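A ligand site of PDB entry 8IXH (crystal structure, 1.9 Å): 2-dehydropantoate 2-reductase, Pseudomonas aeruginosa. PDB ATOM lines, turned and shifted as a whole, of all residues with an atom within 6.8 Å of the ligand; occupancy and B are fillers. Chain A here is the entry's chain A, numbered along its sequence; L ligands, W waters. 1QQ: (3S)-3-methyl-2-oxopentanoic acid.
An oxygen (O45) of the ligand sits close to the backbone carbonyl oxygen of Cys 131 (2.9 Å).
Asn 108 touches the ligand (ND2 to OXT, 3.5 Å).
Phe 132 touches the ligand.
Cys 134 touches the ligand.
CD2 of Tyr 148 touches C49 of the ligand, 3.96 Å away.
Trp 199 touches the ligand (CH2 to C48, 3.3 Å).
Met 260 touches the ligand.
The side-chain amide oxygen (OD1) of Asn 108 sits close to the side-chain amide oxygen (OD1) of Asn 200 (3.4 Å).
The side-chain amide oxygen (OD1) of Asn 204 lies within hydrogen-bond range of the side-chain amide nitrogen (ND2) of Asn 200.
O of Cys 131 lies within hydrogen-bond range of NZ of Lys 196, 2.9 Å away.
The side-chain hydroxyl of Thr 214 lies within hydrogen-bond range of the backbone NH of Tyr 263.
The side-chain hydroxyl (OG1) of Thr 257 sits at hydrogen-bond distance from the indole nitrogen (NE1) of Trp 199 (3.0 Å).
SD of Met 260 sits at hydrogen-bond distance from SG of Cys 134 (3.5 Å).
The backbone carbonyl oxygen (O) of Ala 147 sits at hydrogen-bond distance from the backbone NH (N) of Cys 134 (3.0 Å).
The side-chain hydroxyl (OH) of Tyr 148 sits at hydrogen-bond distance from the backbone carbonyl oxygen (O) of Ala 256, at 3.2 Å.
The side-chain amide nitrogen of Asn 200 is in hydrogen-bond range of an oxygen (OXT) of the ligand, 2.7 Å away.
The side-chain amino group (NZ) of Lys 196 is in salt-bridge range of an oxygen (OXT) of the ligand, 2.9 Å away.
O45 of the ligand is in hydrogen-bond range of N of Ile 133, at 3.0 Å.
O43 of the ligand lies within hydrogen-bond range of OH of Tyr 263 (3.1 Å).
Water W1 lies within hydrogen-bond range of OG of Ser 266 (2.6 Å), OXT of the ligand (3.0 Å), ND2 of Asn 204 (3.0 Å) and ND2 of Asn 200 (3.5 Å).
Water W2 lies within hydrogen-bond range of the backbone carbonyl oxygen of Cys 131 (2.8 Å), an oxygen (O45) of the ligand (3.2 Å), the side-chain amide nitrogen of Asn 108 (3.2 Å) and the side-chain amino group of Lys 196 (3.3 Å).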
ATOM      1  N   ILE A  16     -20.135  26.840  13.744  1.00  0.00           N
ATOM      2  CA  ILE A  16     -21.564  27.104  13.613  1.00  0.00           C
ATOM      3  C   ILE A  16     -21.812  28.406  12.852  1.00  0.00           C
ATOM      4  O   ILE A  16     -22.580  28.446  11.880  1.00  0.00           O
ATOM      5  CB  ILE A  16     -22.229  27.112  15.006  1.00  0.00           C
ATOM      6  CG1 ILE A  16     -22.229  25.707  15.611  1.00  0.00           C
ATOM      7  CG2 ILE A  16     -23.632  27.684  14.934  1.00  0.00           C
ATOM      8  CD1 ILE A  16     -23.243  24.766  14.980  1.00  0.00           C
ATOM      9  N   ASN A 108     -26.450  26.227  22.157  1.00  0.00           N
ATOM     10  CA  ASN A 108     -27.100  25.161  22.899  1.00  0.00           C
ATOM     11  C   ASN A 108     -27.212  25.550  24.369  1.00  0.00           C
ATOM     12  O   ASN A 108     -26.809  26.640  24.781  1.00  0.00           O
ATOM     13  CB  ASN A 108     -26.326  23.856  22.697  1.00  0.00           C
ATOM     14  CG  ASN A 108     -26.365  23.400  21.254  1.00  0.00           C
ATOM     15  OD1 ASN A 108     -27.430  23.329  20.646  1.00  0.00           O
ATOM     16  ND2 ASN A 108     -25.197  23.084  20.696  1.00  0.00           N
ATOM     17  N   LEU A 130     -31.961  26.584  17.715  1.00  0.00           N
ATOM     18  CA  LEU A 130     -31.412  25.294  18.088  1.00  0.00           C
ATOM     19  C   LEU A 130     -31.031  24.550  16.821  1.00  0.00           C
ATOM     20  O   LEU A 130     -31.896  24.126  16.041  1.00  0.00           O
ATOM     21  CB  LEU A 130     -32.407  24.522  18.949  1.00  0.00           C
ATOM     22  CG  LEU A 130     -32.478  25.374  20.224  1.00  0.00           C
ATOM     23  CD1 LEU A 130     -33.915  25.636  20.632  1.00  0.00           C
ATOM     24  CD2 LEU A 130     -31.663  24.775  21.357  1.00  0.00           C
ATOM     25  N   CYS A 131     -29.725  24.398  16.612  1.00  0.00           N
ATOM     26  CA  CYS A 131     -29.196  23.754  15.431  1.00  0.00           C
ATOM     27  C   CYS A 131     -28.924  22.290  15.743  1.00  0.00           C
ATOM     28  O   CYS A 131     -28.167  21.970  16.666  1.00  0.00           O
ATOM     29  CB  CYS A 131     -27.933  24.460  14.963  1.00  0.00           C
ATOM     30  SG  CYS A 131     -28.088  26.268  14.882  1.00  0.00           S
ATOM     31  N   PHE A 132     -29.536  21.399  14.960  1.00  0.00           N
ATOM     32  CA  PHE A 132     -29.227  19.975  14.958  1.00  0.00           C
ATOM     33  C   PHE A 132     -28.303  19.732  13.760  1.00  0.00           C
ATOM     34  O   PHE A 132     -28.766  19.559  12.639  1.00  0.00           O
ATOM     35  CB  PHE A 132     -30.503  19.131  14.855  1.00  0.00           C
ATOM     36  CG  PHE A 132     -31.473  19.328  16.000  1.00  0.00           C
ATOM     37  CD1 PHE A 132     -31.666  18.321  16.935  1.00  0.00           C
ATOM     38  CD2 PHE A 132     -32.228  20.492  16.111  1.00  0.00           C
ATOM     39  CE1 PHE A 132     -32.573  18.477  17.976  1.00  0.00           C
ATOM     40  CE2 PHE A 132     -33.123  20.656  17.154  1.00  0.00           C
ATOM     41  CZ  PHE A 132     -33.298  19.649  18.081  1.00  0.00           C
ATOM     42  N   ILE A 133     -26.990  19.742  14.000  1.00  0.00           N
ATOM     43  CA  ILE A 133     -26.012  19.716  12.935  1.00  0.00           C
ATOM     44  C   ILE A 133     -24.716  19.107  13.449  1.00  0.00           C
ATOM     45  O   ILE A 133     -24.296  19.379  14.582  1.00  0.00           O
ATOM     46  CB  ILE A 133     -25.777  21.134  12.358  1.00  0.00           C
ATOM     47  CG1 ILE A 133     -24.715  21.132  11.262  1.00  0.00           C
ATOM     48  CG2 ILE A 133     -25.404  22.108  13.483  1.00  0.00           C
ATOM     49  CD1 ILE A 133     -24.495  22.498  10.626  1.00  0.00           C
ATOM     50  N   CYS A 134     -24.084  18.287  12.606  1.00  0.00           N
ATOM     51  CA  CYS A 134     -22.766  17.720  12.869  1.00  0.00           C
ATOM     52  C   CYS A 134     -21.765  18.559  12.074  1.00  0.00           C
ATOM     53  O   CYS A 134     -21.656  18.398  10.851  1.00  0.00           O
ATOM     54  CB  CYS A 134     -22.707  16.260  12.434  1.00  0.00           C
ATOM     55  SG  CYS A 134     -23.805  15.164  13.327  1.00  0.00           S
ATOM     56  N   VAL A 135     -21.057  19.451  12.755  1.00  0.00           N
ATOM     57  CA  VAL A 135     -20.122  20.343  12.082  1.00  0.00           C
ATOM     58  C   VAL A 135     -18.983  20.662  13.030  1.00  0.00           C
ATOM     59  O   VAL A 135     -19.170  20.746  14.245  1.00  0.00           O
ATOM     60  CB  VAL A 135     -20.832  21.628  11.582  1.00  0.00           C
ATOM     61  CG1 VAL A 135     -21.152  22.566  12.740  1.00  0.00           C
ATOM     62  CG2 VAL A 135     -19.977  22.327  10.563  1.00  0.00           C
ATOM     63  N   ALA A 147     -23.312  16.082   8.681  1.00  0.00           N
ATOM     64  CA  ALA A 147     -24.699  15.645   8.616  1.00  0.00           C
ATOM     65  C   ALA A 147     -25.625  16.722   9.172  1.00  0.00           C
ATOM     66  O   ALA A 147     -25.207  17.599   9.921  1.00  0.00           O
ATOM     67  CB  ALA A 147     -24.916  14.339   9.381  1.00  0.00           C
ATOM     68  N   TYR A 148     -26.897  16.625   8.780  1.00  0.00           N
ATOM     69  CA  TYR A 148     -28.005  17.417   9.323  1.00  0.00           C
ATOM     70  C   TYR A 148     -27.780  18.899   9.008  1.00  0.00           C
ATOM     71  O   TYR A 148     -27.167  19.243   7.983  1.00  0.00           O
ATOM     72  CB  TYR A 148     -28.175  17.090  10.788  1.00  0.00           C
ATOM     73  CG  TYR A 148     -28.579  15.655  11.035  1.00  0.00           C
ATOM     74  CD1 TYR A 148     -29.767  15.157  10.523  1.00  0.00           C
ATOM     75  CD2 TYR A 148     -27.768  14.799  11.765  1.00  0.00           C
ATOM     76  CE1 TYR A 148     -30.148  13.853  10.738  1.00  0.00           C
ATOM     77  CE2 TYR A 148     -28.143  13.493  11.992  1.00  0.00           C
ATOM     78  CZ  TYR A 148     -29.325  13.017  11.471  1.00  0.00           C
ATOM     79  OH  TYR A 148     -29.703  11.720  11.693  1.00  0.00           O
ATOM     80  N   GLY A 149     -28.271  19.782   9.875  1.00  0.00           N
ATOM     81  CA  GLY A 149     -28.123  21.212   9.672  1.00  0.00           C
ATOM     82  C   GLY A 149     -29.348  22.043   9.999  1.00  0.00           C
ATOM     83  O   GLY A 149     -29.300  23.272   9.986  1.00  0.00           O
ATOM     84  N   LYS A 196     -33.403  20.037  22.666  1.00  0.00           N
ATOM     85  CA  LYS A 196     -32.006  19.871  22.300  1.00  0.00           C
ATOM     86  C   LYS A 196     -31.152  19.417  23.481  1.00  0.00           C
ATOM     87  O   LYS A 196     -30.126  18.752  23.287  1.00  0.00           O
ATOM     88  CB  LYS A 196     -31.456  21.159  21.695  1.00  0.00           C
ATOM     89  CG  LYS A 196     -30.064  21.019  21.090  1.00  0.00           C
ATOM     90  CD  LYS A 196     -30.070  20.104  19.879  1.00  0.00           C
ATOM     91  CE  LYS A 196     -28.659  19.714  19.473  1.00  0.00           C
ATOM     92  NZ  LYS A 196     -27.740  20.887  19.350  1.00  0.00           N
ATOM     93  N   TRP A 199     -30.303  15.732  23.764  1.00  0.00           N
ATOM     94  CA  TRP A 199     -29.153  15.210  23.033  1.00  0.00           C
ATOM     95  C   TRP A 199     -27.840  15.710  23.619  1.00  0.00           C
ATOM     96  O   TRP A 199     -26.919  14.910  23.843  1.00  0.00           O
ATOM     97  CB  TRP A 199     -29.243  15.581  21.539  1.00  0.00           C
ATOM     98  CG  TRP A 199     -28.303  14.763  20.689  1.00  0.00           C
ATOM     99  CD1 TRP A 199     -28.599  13.627  19.986  1.00  0.00           C
ATOM    100  CD2 TRP A 199     -26.901  15.002  20.487  1.00  0.00           C
ATOM    101  NE1 TRP A 199     -27.473  13.155  19.350  1.00  0.00           N
ATOM    102  CE2 TRP A 199     -26.415  13.975  19.643  1.00  0.00           C
ATOM    103  CE3 TRP A 199     -26.012  15.986  20.931  1.00  0.00           C
ATOM    104  CZ2 TRP A 199     -25.085  13.910  19.239  1.00  0.00           C
ATOM    105  CZ3 TRP A 199     -24.682  15.921  20.527  1.00  0.00           C
ATOM    106  CH2 TRP A 199     -24.235  14.886  19.693  1.00  0.00           C
ATOM    107  N   ASN A 200     -27.718  17.009  23.883  1.00  0.00           N
ATOM    108  CA  ASN A 200     -26.419  17.545  24.282  1.00  0.00           C
ATOM    109  C   ASN A 200     -25.997  17.072  25.670  1.00  0.00           C
ATOM    110  O   ASN A 200     -24.809  16.840  25.904  1.00  0.00           O
ATOM    111  CB  ASN A 200     -26.421  19.074  24.239  1.00  0.00           C
ATOM    112  CG  ASN A 200     -26.328  19.631  22.820  1.00  0.00           C
ATOM    113  OD1 ASN A 200     -27.103  20.508  22.446  1.00  0.00           O
ATOM    114  ND2 ASN A 200     -25.363  19.135  22.031  1.00  0.00           N
ATOM    115  N   ASN A 204     -22.584  15.242  24.813  1.00  0.00           N
ATOM    116  CA  ASN A 204     -21.461  16.164  24.997  1.00  0.00           C
ATOM    117  C   ASN A 204     -20.595  15.745  26.183  1.00  0.00           C
ATOM    118  O   ASN A 204     -19.371  15.628  26.062  1.00  0.00           O
ATOM    119  CB  ASN A 204     -21.971  17.592  25.183  1.00  0.00           C
ATOM    120  CG  ASN A 204     -22.441  18.208  23.868  1.00  0.00           C
ATOM    121  OD1 ASN A 204     -23.205  17.598  23.119  1.00  0.00           O
ATOM    122  ND2 ASN A 204     -22.000  19.433  23.586  1.00  0.00           N
ATOM    123  N   THR A 214     -19.568   9.425  18.832  1.00  0.00           N
ATOM    124  CA  THR A 214     -20.927   8.908  18.889  1.00  0.00           C
ATOM    125  C   THR A 214     -20.997   7.416  18.553  1.00  0.00           C
ATOM    126  O   THR A 214     -21.765   6.672  19.172  1.00  0.00           O
ATOM    127  CB  THR A 214     -21.844   9.709  17.955  1.00  0.00           C
ATOM    128  OG1 THR A 214     -21.279   9.729  16.636  1.00  0.00           O
ATOM    129  CG2 THR A 214     -22.035  11.128  18.458  1.00  0.00           C
ATOM    130  N   ALA A 256     -31.667   8.546  15.532  1.00  0.00           N
ATOM    131  CA  ALA A 256     -30.981   9.541  14.697  1.00  0.00           C
ATOM    132  C   ALA A 256     -29.478   9.486  14.887  1.00  0.00           C
ATOM    133  O   ALA A 256     -28.721   9.739  13.943  1.00  0.00           O
ATOM    134  CB  ALA A 256     -31.498  10.939  15.002  1.00  0.00           C
ATOM    135  N   THR A 257     -29.004   9.148  16.096  1.00  0.00           N
ATOM    136  CA  THR A 257     -27.573   9.109  16.346  1.00  0.00           C
ATOM    137  C   THR A 257     -26.943   7.815  15.821  1.00  0.00           C
ATOM    138  O   THR A 257     -25.767   7.818  15.450  1.00  0.00           O
ATOM    139  CB  THR A 257     -27.300   9.286  17.834  1.00  0.00           C
ATOM    140  OG1 THR A 257     -28.121  10.361  18.332  1.00  0.00           O
ATOM    141  CG2 THR A 257     -25.838   9.645  18.069  1.00  0.00           C
ATOM    142  N   MET A 260     -26.327   8.604  12.484  1.00  0.00           N
ATOM    143  CA  MET A 260     -25.371   9.690  12.383  1.00  0.00           C
ATOM    144  C   MET A 260     -23.967   9.147  12.110  1.00  0.00           C
ATOM    145  O   MET A 260     -23.554   8.150  12.714  1.00  0.00           O
ATOM    146  CB  MET A 260     -25.387  10.476  13.697  1.00  0.00           C
ATOM    147  CG  MET A 260     -24.430  11.631  13.790  1.00  0.00           C
ATOM    148  SD  MET A 260     -24.652  12.434  15.394  1.00  0.00           S
ATOM    149  CE  MET A 260     -26.413  12.730  15.363  1.00  0.00           C
ATOM    150  N   TYR A 263     -19.165  10.978  15.170  1.00  0.00           N
ATOM    151  CA  TYR A 263     -19.152  12.415  15.380  1.00  0.00           C
ATOM    152  C   TYR A 263     -18.598  12.753  16.753  1.00  0.00           C
ATOM    153  O   TYR A 263     -18.969  12.129  17.749  1.00  0.00           O
ATOM    154  CB  TYR A 263     -20.563  12.986  15.225  1.00  0.00           C
ATOM    155  CG  TYR A 263     -20.664  14.454  15.571  1.00  0.00           C
ATOM    156  CD1 TYR A 263     -20.132  15.427  14.737  1.00  0.00           C
ATOM    157  CD2 TYR A 263     -21.318  14.866  16.723  1.00  0.00           C
ATOM    158  CE1 TYR A 263     -20.230  16.770  15.056  1.00  0.00           C
ATOM    159  CE2 TYR A 263     -21.413  16.201  17.048  1.00  0.00           C
ATOM    160  CZ  TYR A 263     -20.884  17.153  16.206  1.00  0.00           C
ATOM    161  OH  TYR A 263     -20.990  18.481  16.528  1.00  0.00           O
ATOM    162  N   ARG A 264     -17.716  13.756  16.791  1.00  0.00           N
ATOM    163  CA  ARG A 264     -17.173  14.259  18.041  1.00  0.00           C
ATOM    164  C   ARG A 264     -17.942  15.513  18.433  1.00  0.00           C
ATOM    165  O   ARG A 264     -17.843  16.531  17.718  1.00  0.00           O
ATOM    166  CB  ARG A 264     -15.686  14.557  17.905  1.00  0.00           C
ATOM    167  CG  ARG A 264     -14.800  13.324  17.876  1.00  0.00           C
ATOM    168  CD  ARG A 264     -13.432  13.617  17.261  1.00  0.00           C
ATOM    169  NE  ARG A 264     -12.675  12.387  17.010  1.00  0.00           N
ATOM    170  CZ  ARG A 264     -11.352  12.282  17.095  1.00  0.00           C
ATOM    171  NH1 ARG A 264     -10.619  13.331  17.430  1.00  0.00           N
ATOM    172  NH2 ARG A 264     -10.761  11.122  16.851  1.00  0.00           N
ATOM    173  N   PRO A 265     -18.723  15.498  19.510  1.00  0.00           N
ATOM    174  CA  PRO A 265     -19.455  16.702  19.905  1.00  0.00           C
ATOM    175  C   PRO A 265     -18.511  17.862  20.201  1.00  0.00           C
ATOM    176  O   PRO A 265     -17.317  17.686  20.453  1.00  0.00           O
ATOM    177  CB  PRO A 265     -20.217  16.267  21.167  1.00  0.00           C
ATOM    178  CG  PRO A 265     -20.288  14.764  21.059  1.00  0.00           C
ATOM    179  CD  PRO A 265     -19.015  14.352  20.388  1.00  0.00           C
ATOM    180  N   SER A 266     -19.063  19.084  20.140  1.00  0.00           N
ATOM    181  CA  SER A 266     -18.256  20.280  20.317  1.00  0.00           C
ATOM    182  C   SER A 266     -17.468  20.248  21.634  1.00  0.00           C
ATOM    183  O   SER A 266     -16.310  20.670  21.682  1.00  0.00           O
ATOM    184  CB  SER A 266     -19.134  21.536  20.250  1.00  0.00           C
ATOM    185  OG  SER A 266     -20.085  21.550  21.301  1.00  0.00           O
HETATM  186  C42 1QQ L   1     -24.623  19.139  18.414  1.00  0.00           C
HETATM  187  C44 1QQ L   1     -25.621  18.827  17.297  1.00  0.00           C
HETATM  188  C46 1QQ L   1     -25.702  17.499  16.538  1.00  0.00           C
HETATM  189  C48 1QQ L   1     -24.619  16.497  16.896  1.00  0.00           C
HETATM  190  C47 1QQ L   1     -27.028  16.781  16.784  1.00  0.00           C
HETATM  191  C49 1QQ L   1     -27.502  16.236  15.442  1.00  0.00           C
HETATM  192  O45 1QQ L   1     -26.390  19.671  16.980  1.00  0.00           O
HETATM  193  O43 1QQ L   1     -23.414  18.760  18.375  1.00  0.00           O
HETATM  194  OXT 1QQ L   1     -25.003  19.829  19.400  1.00  0.00           O
HETATM  195  O   HOH W   1     -22.479  20.575  20.799  1.00  0.00           O
HETATM  196  O   HOH W   2     -25.572  22.675  17.538  1.00  0.00           O
